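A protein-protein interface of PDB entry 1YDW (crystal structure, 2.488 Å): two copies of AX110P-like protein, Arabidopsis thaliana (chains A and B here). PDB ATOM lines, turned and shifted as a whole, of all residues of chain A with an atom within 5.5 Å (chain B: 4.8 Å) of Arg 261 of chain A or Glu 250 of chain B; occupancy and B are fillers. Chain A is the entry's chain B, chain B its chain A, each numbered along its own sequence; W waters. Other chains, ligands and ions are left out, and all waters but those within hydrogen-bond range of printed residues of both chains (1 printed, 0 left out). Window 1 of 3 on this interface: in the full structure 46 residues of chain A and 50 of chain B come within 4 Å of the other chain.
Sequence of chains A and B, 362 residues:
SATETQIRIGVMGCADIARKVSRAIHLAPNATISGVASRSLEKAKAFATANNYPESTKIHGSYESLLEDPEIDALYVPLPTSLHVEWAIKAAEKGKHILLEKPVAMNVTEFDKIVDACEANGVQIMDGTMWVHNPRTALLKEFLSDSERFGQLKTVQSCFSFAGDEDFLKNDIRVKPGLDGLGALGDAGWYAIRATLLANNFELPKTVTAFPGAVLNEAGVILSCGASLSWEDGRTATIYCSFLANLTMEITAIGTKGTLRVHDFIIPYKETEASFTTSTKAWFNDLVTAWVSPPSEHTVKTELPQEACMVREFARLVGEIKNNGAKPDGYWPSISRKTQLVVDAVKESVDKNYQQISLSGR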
ATOM      1  N   ILE A 251      20.128  -8.877  25.638  1.00  0.00           N
ATOM      2  CA  ILE A 251      20.339  -7.758  24.737  1.00  0.00           C
ATOM      3  C   ILE A 251      21.148  -8.281  23.552  1.00  0.00           C
ATOM      4  O   ILE A 251      22.236  -8.858  23.727  1.00  0.00           O
ATOM      5  CB  ILE A 251      21.163  -6.623  25.306  1.00  0.00           C
ATOM      6  CG1 ILE A 251      20.616  -6.180  26.632  1.00  0.00           C
ATOM      7  CG2 ILE A 251      21.201  -5.430  24.308  1.00  0.00           C
ATOM      8  CD1 ILE A 251      21.587  -5.177  27.358  1.00  0.00           C
ATOM      9  N   THR A 252      20.632  -8.043  22.351  1.00  0.00           N
ATOM     10  CA  THR A 252      21.450  -8.133  21.141  1.00  0.00           C
ATOM     11  C   THR A 252      21.402  -6.846  20.353  1.00  0.00           C
ATOM     12  O   THR A 252      20.324  -6.457  19.895  1.00  0.00           O
ATOM     13  CB  THR A 252      21.002  -9.263  20.233  1.00  0.00           C
ATOM     14  OG1 THR A 252      21.068 -10.475  20.973  1.00  0.00           O
ATOM     15  CG2 THR A 252      21.963  -9.422  19.069  1.00  0.00           C
ATOM     16  N   ALA A 253      22.571  -6.209  20.180  1.00  0.00           N
ATOM     17  CA  ALA A 253      22.654  -4.938  19.467  1.00  0.00           C
ATOM     18  C   ALA A 253      23.621  -4.949  18.272  1.00  0.00           C
ATOM     19  O   ALA A 253      24.757  -5.355  18.407  1.00  0.00           O
ATOM     20  CB  ALA A 253      22.996  -3.801  20.455  1.00  0.00           C
ATOM     21  N   THR A 259      28.927  -6.009  16.776  1.00  0.00           N
ATOM     22  CA  THR A 259      27.763  -6.678  17.370  1.00  0.00           C
ATOM     23  C   THR A 259      28.047  -6.832  18.839  1.00  0.00           C
ATOM     24  O   THR A 259      29.186  -7.111  19.200  1.00  0.00           O
ATOM     25  CB  THR A 259      27.601  -8.126  16.759  1.00  0.00           C
ATOM     26  OG1 THR A 259      27.428  -8.009  15.337  1.00  0.00           O
ATOM     27  CG2 THR A 259      26.433  -8.854  17.383  1.00  0.00           C
ATOM     28  N   LEU A 260      27.035  -6.636  19.678  1.00  0.00           N
ATOM     29  CA  LEU A 260      27.178  -6.750  21.136  1.00  0.00           C
ATOM     30  C   LEU A 260      26.110  -7.666  21.697  1.00  0.00           C
ATOM     31  O   LEU A 260      24.926  -7.525  21.341  1.00  0.00           O
ATOM     32  CB  LEU A 260      27.029  -5.369  21.793  1.00  0.00           C
ATOM     33  CG  LEU A 260      26.746  -5.428  23.318  1.00  0.00           C
ATOM     34  CD1 LEU A 260      27.953  -5.936  24.024  1.00  0.00           C
ATOM     35  CD2 LEU A 260      26.265  -4.102  23.961  1.00  0.00           C
ATOM     36  N   ARG A 261      26.524  -8.572  22.575  1.00  0.00           N
ATOM     37  CA  ARG A 261      25.594  -9.507  23.202  1.00  0.00           C
ATOM     38  C   ARG A 261      25.807  -9.580  24.689  1.00  0.00           C
ATOM     39  O   ARG A 261      26.958  -9.734  25.201  1.00  0.00           O
ATOM     40  CB  ARG A 261      25.748 -10.952  22.658  1.00  0.00           C
ATOM     41  CG  ARG A 261      24.703 -11.311  21.591  1.00  0.00           C
ATOM     42  CD  ARG A 261      25.296 -12.057  20.386  1.00  0.00           C
ATOM     43  NE  ARG A 261      26.037 -13.252  20.770  1.00  0.00           N
ATOM     44  CZ  ARG A 261      26.976 -13.843  20.026  1.00  0.00           C
ATOM     45  NH1 ARG A 261      27.295 -13.388  18.786  1.00  0.00           N
ATOM     46  NH2 ARG A 261      27.592 -14.911  20.528  1.00  0.00           N
ATOM     47  N   VAL A 262      24.693  -9.551  25.380  1.00  0.00           N
ATOM     48  CA  VAL A 262      24.727  -9.921  26.763  1.00  0.00           C
ATOM     49  C   VAL A 262      23.535 -10.736  27.109  1.00  0.00           C
ATOM     50  O   VAL A 262      22.453 -10.429  26.679  1.00  0.00           O
ATOM     51  CB  VAL A 262      25.023  -8.695  27.740  1.00  0.00           C
ATOM     52  CG1 VAL A 262      24.684  -7.429  27.156  1.00  0.00           C
ATOM     53  CG2 VAL A 262      24.442  -8.906  29.148  1.00  0.00           C
ATOM     54  N   HIS A 263      23.750 -11.811  27.847  1.00  0.00           N
ATOM     55  CA  HIS A 263      22.691 -12.803  28.111  1.00  0.00           C
ATOM     56  C   HIS A 263      22.158 -12.782  29.556  1.00  0.00           C
ATOM     57  O   HIS A 263      21.211 -13.531  29.857  1.00  0.00           O
ATOM     58  CB  HIS A 263      23.203 -14.234  27.845  1.00  0.00           C
ATOM     59  CG  HIS A 263      23.949 -14.409  26.554  1.00  0.00           C
ATOM     60  ND1 HIS A 263      23.317 -14.467  25.327  1.00  0.00           N
ATOM     61  CD2 HIS A 263      25.273 -14.565  26.301  1.00  0.00           C
ATOM     62  CE1 HIS A 263      24.218 -14.636  24.373  1.00  0.00           C
ATOM     63  NE2 HIS A 263      25.413 -14.710  24.936  1.00  0.00           N
ATOM     64  N   SER A 275      29.896 -10.397  32.522  1.00  0.00           N
ATOM     65  CA  SER A 275      30.491 -10.617  31.202  1.00  0.00           C
ATOM     66  C   SER A 275      29.570 -10.177  30.064  1.00  0.00           C
ATOM     67  O   SER A 275      28.341 -10.248  30.160  1.00  0.00           O
ATOM     68  CB  SER A 275      30.937 -12.060  30.996  1.00  0.00           C
ATOM     69  OG  SER A 275      30.889 -12.818  32.199  1.00  0.00           O
ATOM     70  N   PHE A 276      30.185  -9.692  28.996  1.00  0.00           N
ATOM     71  CA  PHE A 276      29.464  -9.361  27.775  1.00  0.00           C
ATOM     72  C   PHE A 276      30.328  -9.863  26.597  1.00  0.00           C
ATOM     73  O   PHE A 276      31.563 -10.096  26.728  1.00  0.00           O
ATOM     74  CB  PHE A 276      29.194  -7.858  27.674  1.00  0.00           C
ATOM     75  CG  PHE A 276      30.447  -7.013  27.659  1.00  0.00           C
ATOM     76  CD1 PHE A 276      30.912  -6.467  26.483  1.00  0.00           C
ATOM     77  CD2 PHE A 276      31.155  -6.776  28.816  1.00  0.00           C
ATOM     78  CE1 PHE A 276      32.067  -5.690  26.447  1.00  0.00           C
ATOM     79  CE2 PHE A 276      32.312  -6.018  28.795  1.00  0.00           C
ATOM     80  CZ  PHE A 276      32.773  -5.457  27.601  1.00  0.00           C
ATOM     81  N   THR A 277      29.690 -10.075  25.451  1.00  0.00           N
ATOM     82  CA  THR A 277      30.416 -10.560  24.300  1.00  0.00           C
ATOM     83  C   THR A 277      30.356  -9.519  23.192  1.00  0.00           C
ATOM     84  O   THR A 277      29.338  -8.840  23.014  1.00  0.00           O
ATOM     85  CB  THR A 277      29.906 -11.965  23.923  1.00  0.00           C
ATOM     86  OG1 THR A 277      30.576 -12.905  24.761  1.00  0.00           O
ATOM     87  CG2 THR A 277      30.175 -12.338  22.476  1.00  0.00           C
ATOM     88  N   THR A 278      31.451  -9.444  22.456  1.00  0.00           N
ATOM     89  CA  THR A 278      31.723  -8.386  21.518  1.00  0.00           C
ATOM     90  C   THR A 278      32.439  -8.957  20.228  1.00  0.00           C
ATOM     91  O   THR A 278      33.271  -9.892  20.287  1.00  0.00           O
ATOM     92  CB  THR A 278      32.510  -7.277  22.307  1.00  0.00           C
ATOM     93  OG1 THR A 278      31.823  -6.016  22.247  1.00  0.00           O
ATOM     94  CG2 THR A 278      33.978  -7.153  21.909  1.00  0.00           C
ATOM     95  N   PRO A 295      33.325 -14.237  18.137  1.00  0.00           N
ATOM     96  CA  PRO A 295      33.214 -13.144  19.073  1.00  0.00           C
ATOM     97  C   PRO A 295      34.209 -13.263  20.224  1.00  0.00           C
ATOM     98  O   PRO A 295      34.659 -14.347  20.538  1.00  0.00           O
ATOM     99  CB  PRO A 295      31.780 -13.302  19.578  1.00  0.00           C
ATOM    100  CG  PRO A 295      31.057 -13.873  18.436  1.00  0.00           C
ATOM    101  CD  PRO A 295      32.004 -14.838  17.833  1.00  0.00           C
ATOM    102  N   GLN B 157      13.119 -16.424  18.141  1.00  0.00           N
ATOM    103  CA  GLN B 157      13.716 -15.207  17.546  1.00  0.00           C
ATOM    104  C   GLN B 157      14.894 -15.659  16.721  1.00  0.00           C
ATOM    105  O   GLN B 157      15.771 -16.422  17.202  1.00  0.00           O
ATOM    106  CB  GLN B 157      14.280 -14.257  18.605  1.00  0.00           C
ATOM    107  CG  GLN B 157      13.311 -13.252  19.281  1.00  0.00           C
ATOM    108  CD  GLN B 157      12.993 -13.550  20.778  1.00  0.00           C
ATOM    109  OE1 GLN B 157      13.644 -14.360  21.433  1.00  0.00           O
ATOM    110  NE2 GLN B 157      11.995 -12.879  21.299  1.00  0.00           N
ATOM    111  N   SER B 158      14.935 -15.167  15.493  1.00  0.00           N
ATOM    112  CA  SER B 158      16.041 -15.456  14.592  1.00  0.00           C
ATOM    113  C   SER B 158      16.475 -14.294  13.686  1.00  0.00           C
ATOM    114  O   SER B 158      15.637 -13.529  13.134  1.00  0.00           O
ATOM    115  CB  SER B 158      15.722 -16.644  13.712  1.00  0.00           C
ATOM    116  OG  SER B 158      16.940 -17.317  13.560  1.00  0.00           O
ATOM    117  N   CYS B 159      17.785 -14.168  13.513  1.00  0.00           N
ATOM    118  CA  CYS B 159      18.242 -13.245  12.523  1.00  0.00           C
ATOM    119  C   CYS B 159      19.530 -13.605  11.824  1.00  0.00           C
ATOM    120  O   CYS B 159      20.252 -14.531  12.210  1.00  0.00           O
ATOM    121  CB  CYS B 159      18.357 -11.868  13.140  1.00  0.00           C
ATOM    122  SG  CYS B 159      19.821 -11.755  14.051  1.00  0.00           S
ATOM    123  N   THR B 248      26.146 -11.578  12.108  1.00  0.00           N
ATOM    124  CA  THR B 248      25.414 -11.972  13.302  1.00  0.00           C
ATOM    125  C   THR B 248      24.432 -12.990  12.828  1.00  0.00           C
ATOM    126  O   THR B 248      23.717 -12.740  11.880  1.00  0.00           O
ATOM    127  CB  THR B 248      24.656 -10.744  13.946  1.00  0.00           C
ATOM    128  OG1 THR B 248      25.618  -9.740  14.301  1.00  0.00           O
ATOM    129  CG2 THR B 248      23.869 -11.128  15.181  1.00  0.00           C
ATOM    130  N   MET B 249      24.411 -14.139  13.492  1.00  0.00           N
ATOM    131  CA  MET B 249      23.524 -15.280  13.130  1.00  0.00           C
ATOM    132  C   MET B 249      23.002 -15.916  14.404  1.00  0.00           C
ATOM    133  O   MET B 249      23.714 -16.769  14.951  1.00  0.00           O
ATOM    134  CB  MET B 249      24.299 -16.408  12.392  1.00  0.00           C
ATOM    135  CG  MET B 249      25.012 -16.007  11.150  1.00  0.00           C
ATOM    136  SD  MET B 249      26.276 -17.407  10.647  1.00  0.00           S
ATOM    137  CE  MET B 249      26.586 -17.962  12.102  1.00  0.00           C
ATOM    138  N   GLU B 250      21.784 -15.587  14.837  1.00  0.00           N
ATOM    139  CA  GLU B 250      21.281 -16.131  16.121  1.00  0.00           C
ATOM    140  C   GLU B 250      20.008 -16.909  15.964  1.00  0.00           C
ATOM    141  O   GLU B 250      19.111 -16.517  15.229  1.00  0.00           O
ATOM    142  CB  GLU B 250      20.938 -15.018  17.116  1.00  0.00           C
ATOM    143  CG  GLU B 250      22.063 -14.099  17.532  1.00  0.00           C
ATOM    144  CD  GLU B 250      22.961 -14.660  18.602  1.00  0.00           C
ATOM    145  OE1 GLU B 250      22.617 -15.703  19.199  1.00  0.00           O
ATOM    146  OE2 GLU B 250      24.024 -14.045  18.858  1.00  0.00           O
ATOM    147  N   ILE B 251      19.885 -17.995  16.693  1.00  0.00           N
ATOM    148  CA  ILE B 251      18.547 -18.540  16.972  1.00  0.00           C
ATOM    149  C   ILE B 251      18.380 -18.446  18.465  1.00  0.00           C
ATOM    150  O   ILE B 251      19.288 -18.805  19.203  1.00  0.00           O
ATOM    151  CB  ILE B 251      18.386 -20.014  16.677  1.00  0.00           C
ATOM    152  CG1 ILE B 251      18.448 -20.271  15.185  1.00  0.00           C
ATOM    153  CG2 ILE B 251      17.040 -20.465  17.227  1.00  0.00           C
ATOM    154  CD1 ILE B 251      18.499 -21.796  14.847  1.00  0.00           C
ATOM    155  N   THR B 252      17.235 -17.951  18.895  1.00  0.00           N
ATOM    156  CA  THR B 252      16.793 -18.078  20.310  1.00  0.00           C
ATOM    157  C   THR B 252      15.377 -18.588  20.353  1.00  0.00           C
ATOM    158  O   THR B 252      14.437 -18.049  19.686  1.00  0.00           O
ATOM    159  CB  THR B 252      16.912 -16.735  21.064  1.00  0.00           C
ATOM    160  OG1 THR B 252      18.298 -16.523  21.356  1.00  0.00           O
ATOM    161  CG2 THR B 252      16.146 -16.759  22.367  1.00  0.00           C
ATOM    162  N   VAL B 262      21.506 -20.418  19.699  1.00  0.00           N
ATOM    163  CA  VAL B 262      22.563 -20.704  18.743  1.00  0.00           C
ATOM    164  C   VAL B 262      23.123 -19.391  18.162  1.00  0.00           C
ATOM    165  O   VAL B 262      22.379 -18.535  17.663  1.00  0.00           O
ATOM    166  CB  VAL B 262      22.058 -21.727  17.674  1.00  0.00           C
ATOM    167  CG1 VAL B 262      23.202 -22.401  16.996  1.00  0.00           C
ATOM    168  CG2 VAL B 262      21.259 -22.795  18.360  1.00  0.00           C
ATOM    169  N   HIS B 263      24.437 -19.241  18.237  1.00  0.00           N
ATOM    170  CA  HIS B 263      25.051 -18.015  17.789  1.00  0.00           C
ATOM    171  C   HIS B 263      25.777 -18.131  16.473  1.00  0.00           C
ATOM    172  O   HIS B 263      26.180 -17.095  15.912  1.00  0.00           O
ATOM    173  CB  HIS B 263      26.100 -17.539  18.780  1.00  0.00           C
ATOM    174  CG  HIS B 263      25.580 -17.375  20.159  1.00  0.00           C
ATOM    175  ND1 HIS B 263      24.541 -16.520  20.464  1.00  0.00           N
ATOM    176  CD2 HIS B 263      25.939 -17.979  21.319  1.00  0.00           C
ATOM    177  CE1 HIS B 263      24.285 -16.605  21.753  1.00  0.00           C
ATOM    178  NE2 HIS B 263      25.128 -17.471  22.295  1.00  0.00           N
ATOM    179  N   PHE B 265      25.466 -21.267  13.223  1.00  0.00           N
ATOM    180  CA  PHE B 265      24.068 -21.754  12.823  1.00  0.00           C
ATOM    181  C   PHE B 265      23.767 -21.750  11.380  1.00  0.00           C
ATOM    182  O   PHE B 265      23.292 -22.727  10.906  1.00  0.00           O
ATOM    183  CB  PHE B 265      22.877 -21.158  13.675  1.00  0.00           C
ATOM    184  CG  PHE B 265      21.710 -20.503  12.868  1.00  0.00           C
ATOM    185  CD1 PHE B 265      20.860 -21.250  12.062  1.00  0.00           C
ATOM    186  CD2 PHE B 265      21.452 -19.111  12.973  1.00  0.00           C
ATOM    187  CE1 PHE B 265      19.776 -20.621  11.318  1.00  0.00           C
ATOM    188  CE2 PHE B 265      20.387 -18.457  12.224  1.00  0.00           C
ATOM    189  CZ  PHE B 265      19.553 -19.232  11.395  1.00  0.00           C
ATOM    190  N   TYR B 269      31.410 -21.787  13.423  1.00  0.00           N
ATOM    191  CA  TYR B 269      32.654 -21.095  13.576  1.00  0.00           C
ATOM    192  C   TYR B 269      33.736 -21.866  12.883  1.00  0.00           C
ATOM    193  O   TYR B 269      34.524 -21.284  12.158  1.00  0.00           O
ATOM    194  CB  TYR B 269      32.978 -20.982  15.073  1.00  0.00           C
ATOM    195  CG  TYR B 269      32.160 -19.943  15.823  1.00  0.00           C
ATOM    196  CD1 TYR B 269      31.777 -18.747  15.209  1.00  0.00           C
ATOM    197  CD2 TYR B 269      31.811 -20.148  17.157  1.00  0.00           C
ATOM    198  CE1 TYR B 269      31.024 -17.795  15.887  1.00  0.00           C
ATOM    199  CE2 TYR B 269      31.061 -19.202  17.868  1.00  0.00           C
ATOM    200  CZ  TYR B 269      30.655 -18.024  17.239  1.00  0.00           C
ATOM    201  OH  TYR B 269      29.903 -17.079  17.974  1.00  0.00           O
HETATM  202  O   HOH W   1      26.140 -14.610  15.891  1.00  0.00           O
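His 263 of chain B touches its own counterpart, His 263 of chain A.
4 positions are printed for both chains.
O of Glu 250 of chain B is in hydrogen-bond range of OG of Ser 158 of chain B (2.9 Å).
O of Glu 250 of chain B sits at hydrogen-bond distance from N of Cys 159 of chain B, 3.2 Å away.
The backbone carbonyl oxygen of Met 249 of chain B sits close to the backbone carbonyl oxygen of His 263 of chain B (2.7 Å).
A ring nitrogen (ND1) of His 263 of chain B lies within hydrogen-bond range of the side-chain carboxylate (OE1) of Glu 250 of chain B, at 2.4 Å.
The backbone carbonyl oxygen (O) of Arg 261 of chain A lies within hydrogen-bond range of the backbone NH (N) of Thr 277 of chain A (2.8 Å).
Water W1 lies within hydrogen-bond range of the backbone carbonyl oxygen of His 263 of chain B, the backbone NH of Met 249 of chain B and the guanidinium group of Arg 261 of chain A.
The side-chain hydroxyl (OG1) of Thr 259 of chain A lies within hydrogen-bond range of the side-chain hydroxyl (OG1) of Thr 248 of chain B, 2.7 Å away.
The guanidinium group of Arg 261 of chain A is in salt-bridge range of the side-chain carboxylate of Glu 250 of chain B (2.9 Å).
A ring nitrogen (ND1) of His 263 of chain B sits close to the guanidinium group of Arg 261 of chain A.
Of chain B, only Glu 250 (2.8 Å) and His 263 (3.2 Å) come within 4 Å of Arg 261 of chain A.
Printed residues of chain B within 4 Å of Thr 259 of chain A: Thr 248 (2.7 Å).
Of the printed residues of chain A, Thr 248 of chain B touches Thr 259 (2.7 Å).
Of the printed residues of chain B, His 263 of chain A touches His 263 (3.3 Å).
The nearest residue of chain B that does not touch Arg 261 of chain A is Tyr 269 of chain B (4.1 Å).
Of the 12 printed residues of chain B, 4 touch a printed residue of chain A.
Printed residues of chain B that touch a printed residue of chain A: Thr 248, Glu 250, His 263 and Tyr 269.
Of the 13 printed residues of chain A, 4 touch a printed residue of chain B.
Hydrophobic or aromatic side chains of chain A that line the printed part of chain B: His 263 and Pro 295.
Among the printed residues, pairs that only touch across the chains: His 263 of chain A with His 263 of chain B (3.3 Å) and Pro 295 of chain A with Tyr 269 of chain B (3.1 Å).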
